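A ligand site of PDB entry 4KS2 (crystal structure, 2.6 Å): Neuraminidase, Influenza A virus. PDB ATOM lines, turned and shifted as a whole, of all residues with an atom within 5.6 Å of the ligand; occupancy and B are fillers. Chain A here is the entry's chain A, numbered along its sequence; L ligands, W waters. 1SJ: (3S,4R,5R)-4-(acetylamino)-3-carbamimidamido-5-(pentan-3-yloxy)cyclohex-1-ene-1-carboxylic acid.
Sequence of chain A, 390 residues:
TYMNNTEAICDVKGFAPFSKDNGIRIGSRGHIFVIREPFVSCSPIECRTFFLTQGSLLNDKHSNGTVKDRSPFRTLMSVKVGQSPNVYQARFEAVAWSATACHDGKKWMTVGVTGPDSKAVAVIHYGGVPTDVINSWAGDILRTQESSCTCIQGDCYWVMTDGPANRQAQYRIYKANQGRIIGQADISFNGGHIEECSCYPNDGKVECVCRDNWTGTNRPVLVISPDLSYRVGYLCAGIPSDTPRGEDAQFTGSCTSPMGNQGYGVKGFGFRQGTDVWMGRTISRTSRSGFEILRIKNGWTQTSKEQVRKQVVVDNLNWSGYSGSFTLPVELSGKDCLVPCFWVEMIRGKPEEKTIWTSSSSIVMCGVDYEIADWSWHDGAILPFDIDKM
The backbone carbonyl oxygen (O) of Asp 69 lies within hydrogen-bond range of a nitrogen (NAD) of the ligand (2.7 Å).
NAD of the ligand is in hydrogen-bond range of O of Trp 97 (2.8 Å).
NH1 of Arg 288 lies within salt-bridge range of OAG of the ligand (2.9 Å).
The side-chain carboxylate (OE2) of Glu 37 lies within salt-bridge range of a nitrogen (NAM) of the ligand (3.5 Å).
The side-chain carboxylate (OD1) of Asp 69 is in salt-bridge range of a nitrogen (NAM) of the ligand (3.0 Å).
The guanidinium group of Arg 211 lies within salt-bridge range of an oxygen (OAG) of the ligand, 3.4 Å away.
NH2 of Arg 36 is in salt-bridge range of OAH of the ligand (2.6 Å).
The side-chain carboxylate (OE2) of Glu 146 is in salt-bridge range of a nitrogen (NAE) of the ligand (3.6 Å).
The guanidinium group (NH2) of Arg 70 lies within hydrogen-bond range of an oxygen (OAF) of the ligand, at 3.0 Å.
O of Ile 141 sits at hydrogen-bond distance from NH2 of Arg 143, at 2.7 Å.
The side-chain hydroxyl (OH) of Tyr 322 sits at hydrogen-bond distance from the side-chain carboxylate (OE2) of Glu 196 (2.7 Å).
NH1 of Arg 288 is in hydrogen-bond range of O of Gly 265, 3.1 Å away.
The guanidinium group (NE) of Arg 36 lies within salt-bridge range of the side-chain carboxylate (OE2) of Glu 37.
O of Arg 211 sits at hydrogen-bond distance from N of Glu 195 (2.6 Å).
The side-chain hydroxyl (OH) of Tyr 322 is in hydrogen-bond range of the guanidinium group (NH2) of Arg 211 (3.1 Å).
O of Gly 265 lies within hydrogen-bond range of NH1 of Arg 211 (2.9 Å).
The backbone NH (N) of Arg 36 sits at hydrogen-bond distance from the backbone carbonyl oxygen (O) of Leu 52, 3.0 Å away.
NH2 of Arg 74 lies close to NAD of the ligand (3.3 Å).
Merely in contact with the ligand: Ser 98, Ile 141, Arg 143, Ala 165, Glu 195, Glu 196, Asn 213 and Tyr 322.
17 residues have an atom within 4 Å of the ligand: Arg 36, Glu 37, Asp 69, Arg 70, Arg 74, Trp 97, Ser 98, Ile 141, Arg 143, Glu 146, Ala 165, Glu 195, Glu 196, Arg 211, Asn 213, Arg 288 and Tyr 322.
The nearest printed residue that does not touch the ligand is Leu 52 (4.2 Å).
Water W1 lies within hydrogen-bond range of OE2 of Glu 37 (2.6 Å), OD1 of Asp 69 (2.7 Å) and NAM of the ligand (2.8 Å).
Water W2 lies within hydrogen-bond range of the side-chain carboxylate of Glu 196 (2.6 Å), the side-chain carboxylate of Glu 146 (2.7 Å) and a nitrogen (NAN) of the ligand (3.1 Å).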
ATOM      1  N   ARG A  36      -0.726  -7.769   9.331  1.00  0.00           N
ATOM      2  CA  ARG A  36       0.526  -7.802   8.587  1.00  0.00           C
ATOM      3  C   ARG A  36       0.891  -6.385   8.144  1.00  0.00           C
ATOM      4  O   ARG A  36       0.034  -5.500   8.138  1.00  0.00           O
ATOM      5  CB  ARG A  36       0.392  -8.719   7.367  1.00  0.00           C
ATOM      6  CG  ARG A  36       0.940 -10.118   7.594  1.00  0.00           C
ATOM      7  CD  ARG A  36       1.954 -10.498   6.524  1.00  0.00           C
ATOM      8  NE  ARG A  36       3.205  -9.780   6.682  1.00  0.00           N
ATOM      9  CZ  ARG A  36       4.173  -9.748   5.771  1.00  0.00           C
ATOM     10  NH1 ARG A  36       5.283  -9.063   6.009  1.00  0.00           N
ATOM     11  NH2 ARG A  36       4.024 -10.390   4.623  1.00  0.00           N
ATOM     12  N   GLU A  37       2.144  -6.185   7.786  1.00  0.00           N
ATOM     13  CA  GLU A  37       2.631  -4.850   7.380  1.00  0.00           C
ATOM     14  C   GLU A  37       2.507  -3.681   8.355  1.00  0.00           C
ATOM     15  O   GLU A  37       2.065  -2.610   7.966  1.00  0.00           O
ATOM     16  CB  GLU A  37       1.897  -4.470   6.077  1.00  0.00           C
ATOM     17  CG  GLU A  37       2.084  -5.418   4.934  1.00  0.00           C
ATOM     18  CD  GLU A  37       1.230  -6.653   5.047  1.00  0.00           C
ATOM     19  OE1 GLU A  37       0.120  -6.551   5.588  1.00  0.00           O
ATOM     20  OE2 GLU A  37       1.667  -7.728   4.600  1.00  0.00           O
ATOM     21  N   LEU A  52      -2.233  -3.434   9.040  1.00  0.00           N
ATOM     22  CA  LEU A  52      -3.322  -3.957   8.256  1.00  0.00           C
ATOM     23  C   LEU A  52      -3.903  -5.162   8.986  1.00  0.00           C
ATOM     24  O   LEU A  52      -3.210  -6.144   9.200  1.00  0.00           O
ATOM     25  CB  LEU A  52      -2.835  -4.381   6.885  1.00  0.00           C
ATOM     26  CG  LEU A  52      -2.180  -3.277   6.069  1.00  0.00           C
ATOM     27  CD1 LEU A  52      -1.799  -3.800   4.690  1.00  0.00           C
ATOM     28  CD2 LEU A  52      -3.116  -2.085   5.963  1.00  0.00           C
ATOM     29  N   LYS A  68      -3.078 -14.977   3.185  1.00  0.00           N
ATOM     30  CA  LYS A  68      -3.538 -14.270   1.997  1.00  0.00           C
ATOM     31  C   LYS A  68      -3.218 -12.791   2.104  1.00  0.00           C
ATOM     32  O   LYS A  68      -3.359 -12.192   3.158  1.00  0.00           O
ATOM     33  CB  LYS A  68      -5.021 -14.515   1.699  1.00  0.00           C
ATOM     34  CG  LYS A  68      -5.576 -13.871   0.428  1.00  0.00           C
ATOM     35  CD  LYS A  68      -7.062 -14.253   0.244  1.00  0.00           C
ATOM     36  CE  LYS A  68      -7.695 -13.620  -1.000  1.00  0.00           C
ATOM     37  NZ  LYS A  68      -9.144 -13.996  -1.162  1.00  0.00           N
ATOM     38  N   ASP A  69      -2.773 -12.217   0.998  1.00  0.00           N
ATOM     39  CA  ASP A  69      -2.344 -10.824   0.981  1.00  0.00           C
ATOM     40  C   ASP A  69      -3.503  -9.858   0.964  1.00  0.00           C
ATOM     41  O   ASP A  69      -3.550  -8.925   1.741  1.00  0.00           O
ATOM     42  CB  ASP A  69      -1.473 -10.570  -0.229  1.00  0.00           C
ATOM     43  CG  ASP A  69      -0.107 -11.141  -0.063  1.00  0.00           C
ATOM     44  OD1 ASP A  69       0.542 -10.827   0.946  1.00  0.00           O
ATOM     45  OD2 ASP A  69       0.306 -11.915  -0.946  1.00  0.00           O
ATOM     46  N   ARG A  70      -4.450 -10.077   0.056  1.00  0.00           N
ATOM     47  CA  ARG A  70      -5.519  -9.125  -0.123  1.00  0.00           C
ATOM     48  C   ARG A  70      -6.841  -9.773   0.141  1.00  0.00           C
ATOM     49  O   ARG A  70      -7.056 -10.927  -0.183  1.00  0.00           O
ATOM     50  CB  ARG A  70      -5.463  -8.539  -1.537  1.00  0.00           C
ATOM     51  CG  ARG A  70      -4.085  -7.980  -1.883  1.00  0.00           C
ATOM     52  CD  ARG A  70      -3.921  -7.599  -3.358  1.00  0.00           C
ATOM     53  NE  ARG A  70      -4.093  -8.743  -4.242  1.00  0.00           N
ATOM     54  CZ  ARG A  70      -3.139  -9.627  -4.521  1.00  0.00           C
ATOM     55  NH1 ARG A  70      -3.376 -10.632  -5.342  1.00  0.00           N
ATOM     56  NH2 ARG A  70      -1.947  -9.524  -3.958  1.00  0.00           N
ATOM     57  N   ARG A  74      -9.690  -6.721   5.083  1.00  0.00           N
ATOM     58  CA  ARG A  74      -8.463  -6.091   5.573  1.00  0.00           C
ATOM     59  C   ARG A  74      -8.613  -4.592   5.734  1.00  0.00           C
ATOM     60  O   ARG A  74      -8.971  -3.898   4.801  1.00  0.00           O
ATOM     61  CB  ARG A  74      -7.273  -6.384   4.670  1.00  0.00           C
ATOM     62  CG  ARG A  74      -6.811  -7.830   4.701  1.00  0.00           C
ATOM     63  CD  ARG A  74      -5.395  -7.974   4.169  1.00  0.00           C
ATOM     64  NE  ARG A  74      -4.389  -7.658   5.166  1.00  0.00           N
ATOM     65  CZ  ARG A  74      -3.180  -8.207   5.201  1.00  0.00           C
ATOM     66  NH1 ARG A  74      -2.309  -7.878   6.133  1.00  0.00           N
ATOM     67  NH2 ARG A  74      -2.841  -9.095   4.272  1.00  0.00           N
ATOM     68  N   TRP A  97      -5.798  -3.156   2.068  1.00  0.00           N
ATOM     69  CA  TRP A  97      -4.840  -4.262   2.087  1.00  0.00           C
ATOM     70  C   TRP A  97      -3.434  -3.830   1.644  1.00  0.00           C
ATOM     71  O   TRP A  97      -2.544  -4.643   1.470  1.00  0.00           O
ATOM     72  CB  TRP A  97      -5.326  -5.481   1.318  1.00  0.00           C
ATOM     73  CG  TRP A  97      -6.037  -5.223   0.042  1.00  0.00           C
ATOM     74  CD1 TRP A  97      -7.343  -5.486  -0.231  1.00  0.00           C
ATOM     75  CD2 TRP A  97      -5.486  -4.652  -1.146  1.00  0.00           C
ATOM     76  NE1 TRP A  97      -7.653  -5.119  -1.508  1.00  0.00           N
ATOM     77  CE2 TRP A  97      -6.526  -4.612  -2.099  1.00  0.00           C
ATOM     78  CE3 TRP A  97      -4.217  -4.193  -1.520  1.00  0.00           C
ATOM     79  CZ2 TRP A  97      -6.342  -4.106  -3.395  1.00  0.00           C
ATOM     80  CZ3 TRP A  97      -4.032  -3.698  -2.807  1.00  0.00           C
ATOM     81  CH2 TRP A  97      -5.087  -3.664  -3.726  1.00  0.00           C
ATOM     82  N   SER A  98      -3.278  -2.513   1.489  1.00  0.00           N
ATOM     83  CA  SER A  98      -2.007  -1.859   1.226  1.00  0.00           C
ATOM     84  C   SER A  98      -2.209  -0.417   1.663  1.00  0.00           C
ATOM     85  O   SER A  98      -3.252   0.168   1.411  1.00  0.00           O
ATOM     86  CB  SER A  98      -1.659  -1.930  -0.263  1.00  0.00           C
ATOM     87  OG  SER A  98      -0.506  -1.165  -0.565  1.00  0.00           O
ATOM     88  N   ILE A 141      -3.089  -4.482  -9.278  1.00  0.00           N
ATOM     89  CA  ILE A 141      -2.755  -4.344  -7.857  1.00  0.00           C
ATOM     90  C   ILE A 141      -2.152  -3.005  -7.389  1.00  0.00           C
ATOM     91  O   ILE A 141      -1.093  -2.988  -6.778  1.00  0.00           O
ATOM     92  CB  ILE A 141      -1.832  -5.493  -7.382  1.00  0.00           C
ATOM     93  CG1 ILE A 141      -2.522  -6.835  -7.568  1.00  0.00           C
ATOM     94  CG2 ILE A 141      -1.441  -5.280  -5.922  1.00  0.00           C
ATOM     95  CD1 ILE A 141      -1.587  -8.018  -7.523  1.00  0.00           C
ATOM     96  N   LEU A 142      -2.828  -1.907  -7.679  1.00  0.00           N
ATOM     97  CA  LEU A 142      -2.414  -0.617  -7.152  1.00  0.00           C
ATOM     98  C   LEU A 142      -2.015  -0.706  -5.691  1.00  0.00           C
ATOM     99  O   LEU A 142      -2.811  -1.161  -4.862  1.00  0.00           O
ATOM    100  CB  LEU A 142      -3.485   0.446  -7.351  1.00  0.00           C
ATOM    101  CG  LEU A 142      -3.194   1.802  -6.707  1.00  0.00           C
ATOM    102  CD1 LEU A 142      -2.090   2.498  -7.468  1.00  0.00           C
ATOM    103  CD2 LEU A 142      -4.440   2.669  -6.645  1.00  0.00           C
ATOM    104  N   ARG A 143      -0.795  -0.301  -5.361  1.00  0.00           N
ATOM    105  CA  ARG A 143      -0.289  -0.455  -3.993  1.00  0.00           C
ATOM    106  C   ARG A 143       0.568   0.716  -3.544  1.00  0.00           C
ATOM    107  O   ARG A 143       0.833   1.631  -4.310  1.00  0.00           O
ATOM    108  CB  ARG A 143       0.494  -1.770  -3.865  1.00  0.00           C
ATOM    109  CG  ARG A 143       1.480  -2.018  -4.992  1.00  0.00           C
ATOM    110  CD  ARG A 143       1.738  -3.500  -5.185  1.00  0.00           C
ATOM    111  NE  ARG A 143       2.731  -3.756  -6.222  1.00  0.00           N
ATOM    112  CZ  ARG A 143       2.450  -3.835  -7.521  1.00  0.00           C
ATOM    113  NH1 ARG A 143       3.416  -4.063  -8.399  1.00  0.00           N
ATOM    114  NH2 ARG A 143       1.200  -3.696  -7.942  1.00  0.00           N
ATOM    115  N   GLU A 146       3.443   0.854   2.473  1.00  0.00           N
ATOM    116  CA  GLU A 146       3.334  -0.098   3.575  1.00  0.00           C
ATOM    117  C   GLU A 146       4.189   0.430   4.723  1.00  0.00           C
ATOM    118  O   GLU A 146       4.647  -0.327   5.575  1.00  0.00           O
ATOM    119  CB  GLU A 146       3.761  -1.493   3.153  1.00  0.00           C
ATOM    120  CG  GLU A 146       3.060  -2.010   1.901  1.00  0.00           C
ATOM    121  CD  GLU A 146       1.546  -1.968   2.005  1.00  0.00           C
ATOM    122  OE1 GLU A 146       1.034  -1.771   3.117  1.00  0.00           O
ATOM    123  OE2 GLU A 146       0.876  -2.140   0.969  1.00  0.00           O
ATOM    124  N   ALA A 165       4.257  -7.714 -10.458  1.00  0.00           N
ATOM    125  CA  ALA A 165       5.110  -7.809  -9.284  1.00  0.00           C
ATOM    126  C   ALA A 165       6.420  -8.510  -9.626  1.00  0.00           C
ATOM    127  O   ALA A 165       7.298  -8.627  -8.773  1.00  0.00           O
ATOM    128  CB  ALA A 165       4.403  -8.546  -8.165  1.00  0.00           C
ATOM    129  N   GLU A 195       8.991  -1.138  -5.332  1.00  0.00           N
ATOM    130  CA  GLU A 195       7.864  -1.548  -4.487  1.00  0.00           C
ATOM    131  C   GLU A 195       8.053  -1.063  -3.060  1.00  0.00           C
ATOM    132  O   GLU A 195       9.181  -1.026  -2.575  1.00  0.00           O
ATOM    133  CB  GLU A 195       7.733  -3.072  -4.448  1.00  0.00           C
ATOM    134  CG  GLU A 195       7.540  -3.755  -5.791  1.00  0.00           C
ATOM    135  CD  GLU A 195       6.101  -3.779  -6.243  1.00  0.00           C
ATOM    136  OE1 GLU A 195       5.867  -4.101  -7.428  1.00  0.00           O
ATOM    137  OE2 GLU A 195       5.214  -3.470  -5.422  1.00  0.00           O
ATOM    138  N   GLU A 196       6.966  -0.677  -2.404  1.00  0.00           N
ATOM    139  CA  GLU A 196       6.954  -0.472  -0.954  1.00  0.00           C
ATOM    140  C   GLU A 196       8.099   0.399  -0.439  1.00  0.00           C
ATOM    141  O   GLU A 196       8.878  -0.040   0.407  1.00  0.00           O
ATOM    142  CB  GLU A 196       6.970  -1.820  -0.232  1.00  0.00           C
ATOM    143  CG  GLU A 196       5.873  -2.745  -0.685  1.00  0.00           C
ATOM    144  CD  GLU A 196       6.015  -4.153  -0.171  1.00  0.00           C
ATOM    145  OE1 GLU A 196       7.089  -4.523   0.318  1.00  0.00           O
ATOM    146  OE2 GLU A 196       5.033  -4.907  -0.251  1.00  0.00           O
ATOM    147  N   ARG A 211      12.023  -1.299  -2.732  1.00  0.00           N
ATOM    148  CA  ARG A 211      12.168  -2.729  -2.954  1.00  0.00           C
ATOM    149  C   ARG A 211      12.057  -3.064  -4.439  1.00  0.00           C
ATOM    150  O   ARG A 211      11.157  -2.597  -5.137  1.00  0.00           O
ATOM    151  CB  ARG A 211      11.104  -3.499  -2.160  1.00  0.00           C
ATOM    152  CG  ARG A 211      10.919  -4.959  -2.528  1.00  0.00           C
ATOM    153  CD  ARG A 211       9.755  -5.569  -1.756  1.00  0.00           C
ATOM    154  NE  ARG A 211       9.520  -6.963  -2.105  1.00  0.00           N
ATOM    155  CZ  ARG A 211       8.626  -7.757  -1.519  1.00  0.00           C
ATOM    156  NH1 ARG A 211       8.491  -9.021  -1.899  1.00  0.00           N
ATOM    157  NH2 ARG A 211       7.851  -7.284  -0.539  1.00  0.00           N
ATOM    158  N   ASN A 213      11.360  -6.027  -6.762  1.00  0.00           N
ATOM    159  CA  ASN A 213      10.835  -7.379  -6.736  1.00  0.00           C
ATOM    160  C   ASN A 213      11.043  -8.094  -8.058  1.00  0.00           C
ATOM    161  O   ASN A 213      10.527  -9.183  -8.281  1.00  0.00           O
ATOM    162  CB  ASN A 213       9.376  -7.385  -6.338  1.00  0.00           C
ATOM    163  CG  ASN A 213       8.996  -8.620  -5.556  1.00  0.00           C
ATOM    164  OD1 ASN A 213       9.583  -8.922  -4.520  1.00  0.00           O
ATOM    165  ND2 ASN A 213       8.005  -9.345  -6.053  1.00  0.00           N
ATOM    166  N   TYR A 264      12.461 -11.819  -6.509  1.00  0.00           N
ATOM    167  CA  TYR A 264      11.813 -11.712  -5.205  1.00  0.00           C
ATOM    168  C   TYR A 264      12.250 -10.486  -4.375  1.00  0.00           C
ATOM    169  O   TYR A 264      12.862  -9.540  -4.916  1.00  0.00           O
ATOM    170  CB  TYR A 264      11.987 -13.025  -4.433  1.00  0.00           C
ATOM    171  CG  TYR A 264      11.001 -13.250  -3.302  1.00  0.00           C
ATOM    172  CD1 TYR A 264       9.685 -12.873  -3.416  1.00  0.00           C
ATOM    173  CD2 TYR A 264      11.406 -13.871  -2.124  1.00  0.00           C
ATOM    174  CE1 TYR A 264       8.775 -13.079  -2.372  1.00  0.00           C
ATOM    175  CE2 TYR A 264      10.534 -14.091  -1.088  1.00  0.00           C
ATOM    176  CZ  TYR A 264       9.207 -13.694  -1.220  1.00  0.00           C
ATOM    177  OH  TYR A 264       8.325 -13.912  -0.182  1.00  0.00           O
ATOM    178  N   GLY A 265      11.958 -10.487  -3.081  1.00  0.00           N
ATOM    179  CA  GLY A 265      12.349  -9.405  -2.200  1.00  0.00           C
ATOM    180  C   GLY A 265      11.590  -9.287  -0.894  1.00  0.00           C
ATOM    181  O   GLY A 265      10.753 -10.134  -0.554  1.00  0.00           O
ATOM    182  N   VAL A 266      11.888  -8.220  -0.157  1.00  0.00           N
ATOM    183  CA  VAL A 266      11.193  -7.869   1.083  1.00  0.00           C
ATOM    184  C   VAL A 266      11.297  -6.375   1.284  1.00  0.00           C
ATOM    185  O   VAL A 266      12.280  -5.756   0.885  1.00  0.00           O
ATOM    186  CB  VAL A 266      11.812  -8.591   2.310  1.00  0.00           C
ATOM    187  CG1 VAL A 266      13.162  -7.988   2.664  1.00  0.00           C
ATOM    188  CG2 VAL A 266      10.860  -8.526   3.503  1.00  0.00           C
ATOM    189  N   ARG A 288      13.585 -14.963   5.748  1.00  0.00           N
ATOM    190  CA  ARG A 288      13.239 -13.758   6.472  1.00  0.00           C
ATOM    191  C   ARG A 288      13.517 -13.894   7.968  1.00  0.00           C
ATOM    192  O   ARG A 288      12.625 -13.755   8.811  1.00  0.00           O
ATOM    193  CB  ARG A 288      11.793 -13.353   6.201  1.00  0.00           C
ATOM    194  CG  ARG A 288      11.575 -12.838   4.792  1.00  0.00           C
ATOM    195  CD  ARG A 288      10.113 -12.582   4.526  1.00  0.00           C
ATOM    196  NE  ARG A 288       9.909 -11.904   3.245  1.00  0.00           N
ATOM    197  CZ  ARG A 288       8.726 -11.450   2.829  1.00  0.00           C
ATOM    198  NH1 ARG A 288       8.638 -10.842   1.658  1.00  0.00           N
ATOM    199  NH2 ARG A 288       7.652 -11.597   3.589  1.00  0.00           N
ATOM    200  N   TYR A 322       9.485  -7.535   7.275  1.00  0.00           N
ATOM    201  CA  TYR A 322       9.497  -6.130   6.863  1.00  0.00           C
ATOM    202  C   TYR A 322      10.238  -5.204   7.837  1.00  0.00           C
ATOM    203  O   TYR A 322      10.431  -5.501   9.005  1.00  0.00           O
ATOM    204  CB  TYR A 322       8.063  -5.624   6.650  1.00  0.00           C
ATOM    205  CG  TYR A 322       7.441  -5.920   5.309  1.00  0.00           C
ATOM    206  CD1 TYR A 322       7.766  -7.072   4.610  1.00  0.00           C
ATOM    207  CD2 TYR A 322       6.529  -5.057   4.742  1.00  0.00           C
ATOM    208  CE1 TYR A 322       7.191  -7.339   3.382  1.00  0.00           C
ATOM    209  CE2 TYR A 322       5.956  -5.314   3.524  1.00  0.00           C
ATOM    210  CZ  TYR A 322       6.287  -6.456   2.844  1.00  0.00           C
ATOM    211  OH  TYR A 322       5.728  -6.694   1.633  1.00  0.00           O
HETATM  212  CAA 1SJ L   1       6.326  -7.157  -4.393  1.00  0.00           C
HETATM  213  CAJ 1SJ L   1       5.631  -6.485  -3.176  1.00  0.00           C
HETATM  214  CAT 1SJ L   1       4.088  -6.489  -3.342  1.00  0.00           C
HETATM  215  CAK 1SJ L   1       3.712  -6.393  -4.848  1.00  0.00           C
HETATM  216  CAB 1SJ L   1       2.366  -7.075  -5.140  1.00  0.00           C
HETATM  217  OAO 1SJ L   1       3.475  -7.654  -2.738  1.00  0.00           O
HETATM  218  CAV 1SJ L   1       3.450  -7.569  -1.336  1.00  0.00           C
HETATM  219  CAL 1SJ L   1       4.341  -8.684  -0.834  1.00  0.00           C
HETATM  220  CAS 1SJ L   1       4.120  -9.053   0.510  1.00  0.00           C
HETATM  221  CAR 1SJ L   1       5.112  -9.906   1.060  1.00  0.00           C
HETATM  222  OAH 1SJ L   1       4.975 -10.472   2.165  1.00  0.00           O
HETATM  223  OAG 1SJ L   1       6.165 -10.105   0.440  1.00  0.00           O
HETATM  224  CAI 1SJ L   1       2.994  -8.611   1.245  1.00  0.00           C
HETATM  225  CAU 1SJ L   1       2.037  -7.711   0.738  1.00  0.00           C
HETATM  226  NAM 1SJ L   1       0.638  -7.891   1.228  1.00  0.00           N
HETATM  227  CAQ 1SJ L   1      -0.235  -6.895   1.540  1.00  0.00           C
HETATM  228  NAE 1SJ L   1       0.119  -5.628   1.427  1.00  0.00           N
HETATM  229  NAD 1SJ L   1      -1.483  -7.164   1.959  1.00  0.00           N
HETATM  230  CAW 1SJ L   1       2.016  -7.714  -0.788  1.00  0.00           C
HETATM  231  NAN 1SJ L   1       1.191  -6.553  -1.191  1.00  0.00           N
HETATM  232  CAP 1SJ L   1      -0.038  -6.621  -1.747  1.00  0.00           C
HETATM  233  OAF 1SJ L   1      -0.616  -7.674  -1.999  1.00  0.00           O
HETATM  234  CAC 1SJ L   1      -0.687  -5.305  -2.075  1.00  0.00           C
HETATM  235  O   HOH W   1       0.538  -9.679   3.335  1.00  0.00           O
HETATM  236  O   HOH W   2       2.529  -4.101   0.067  1.00  0.00           O
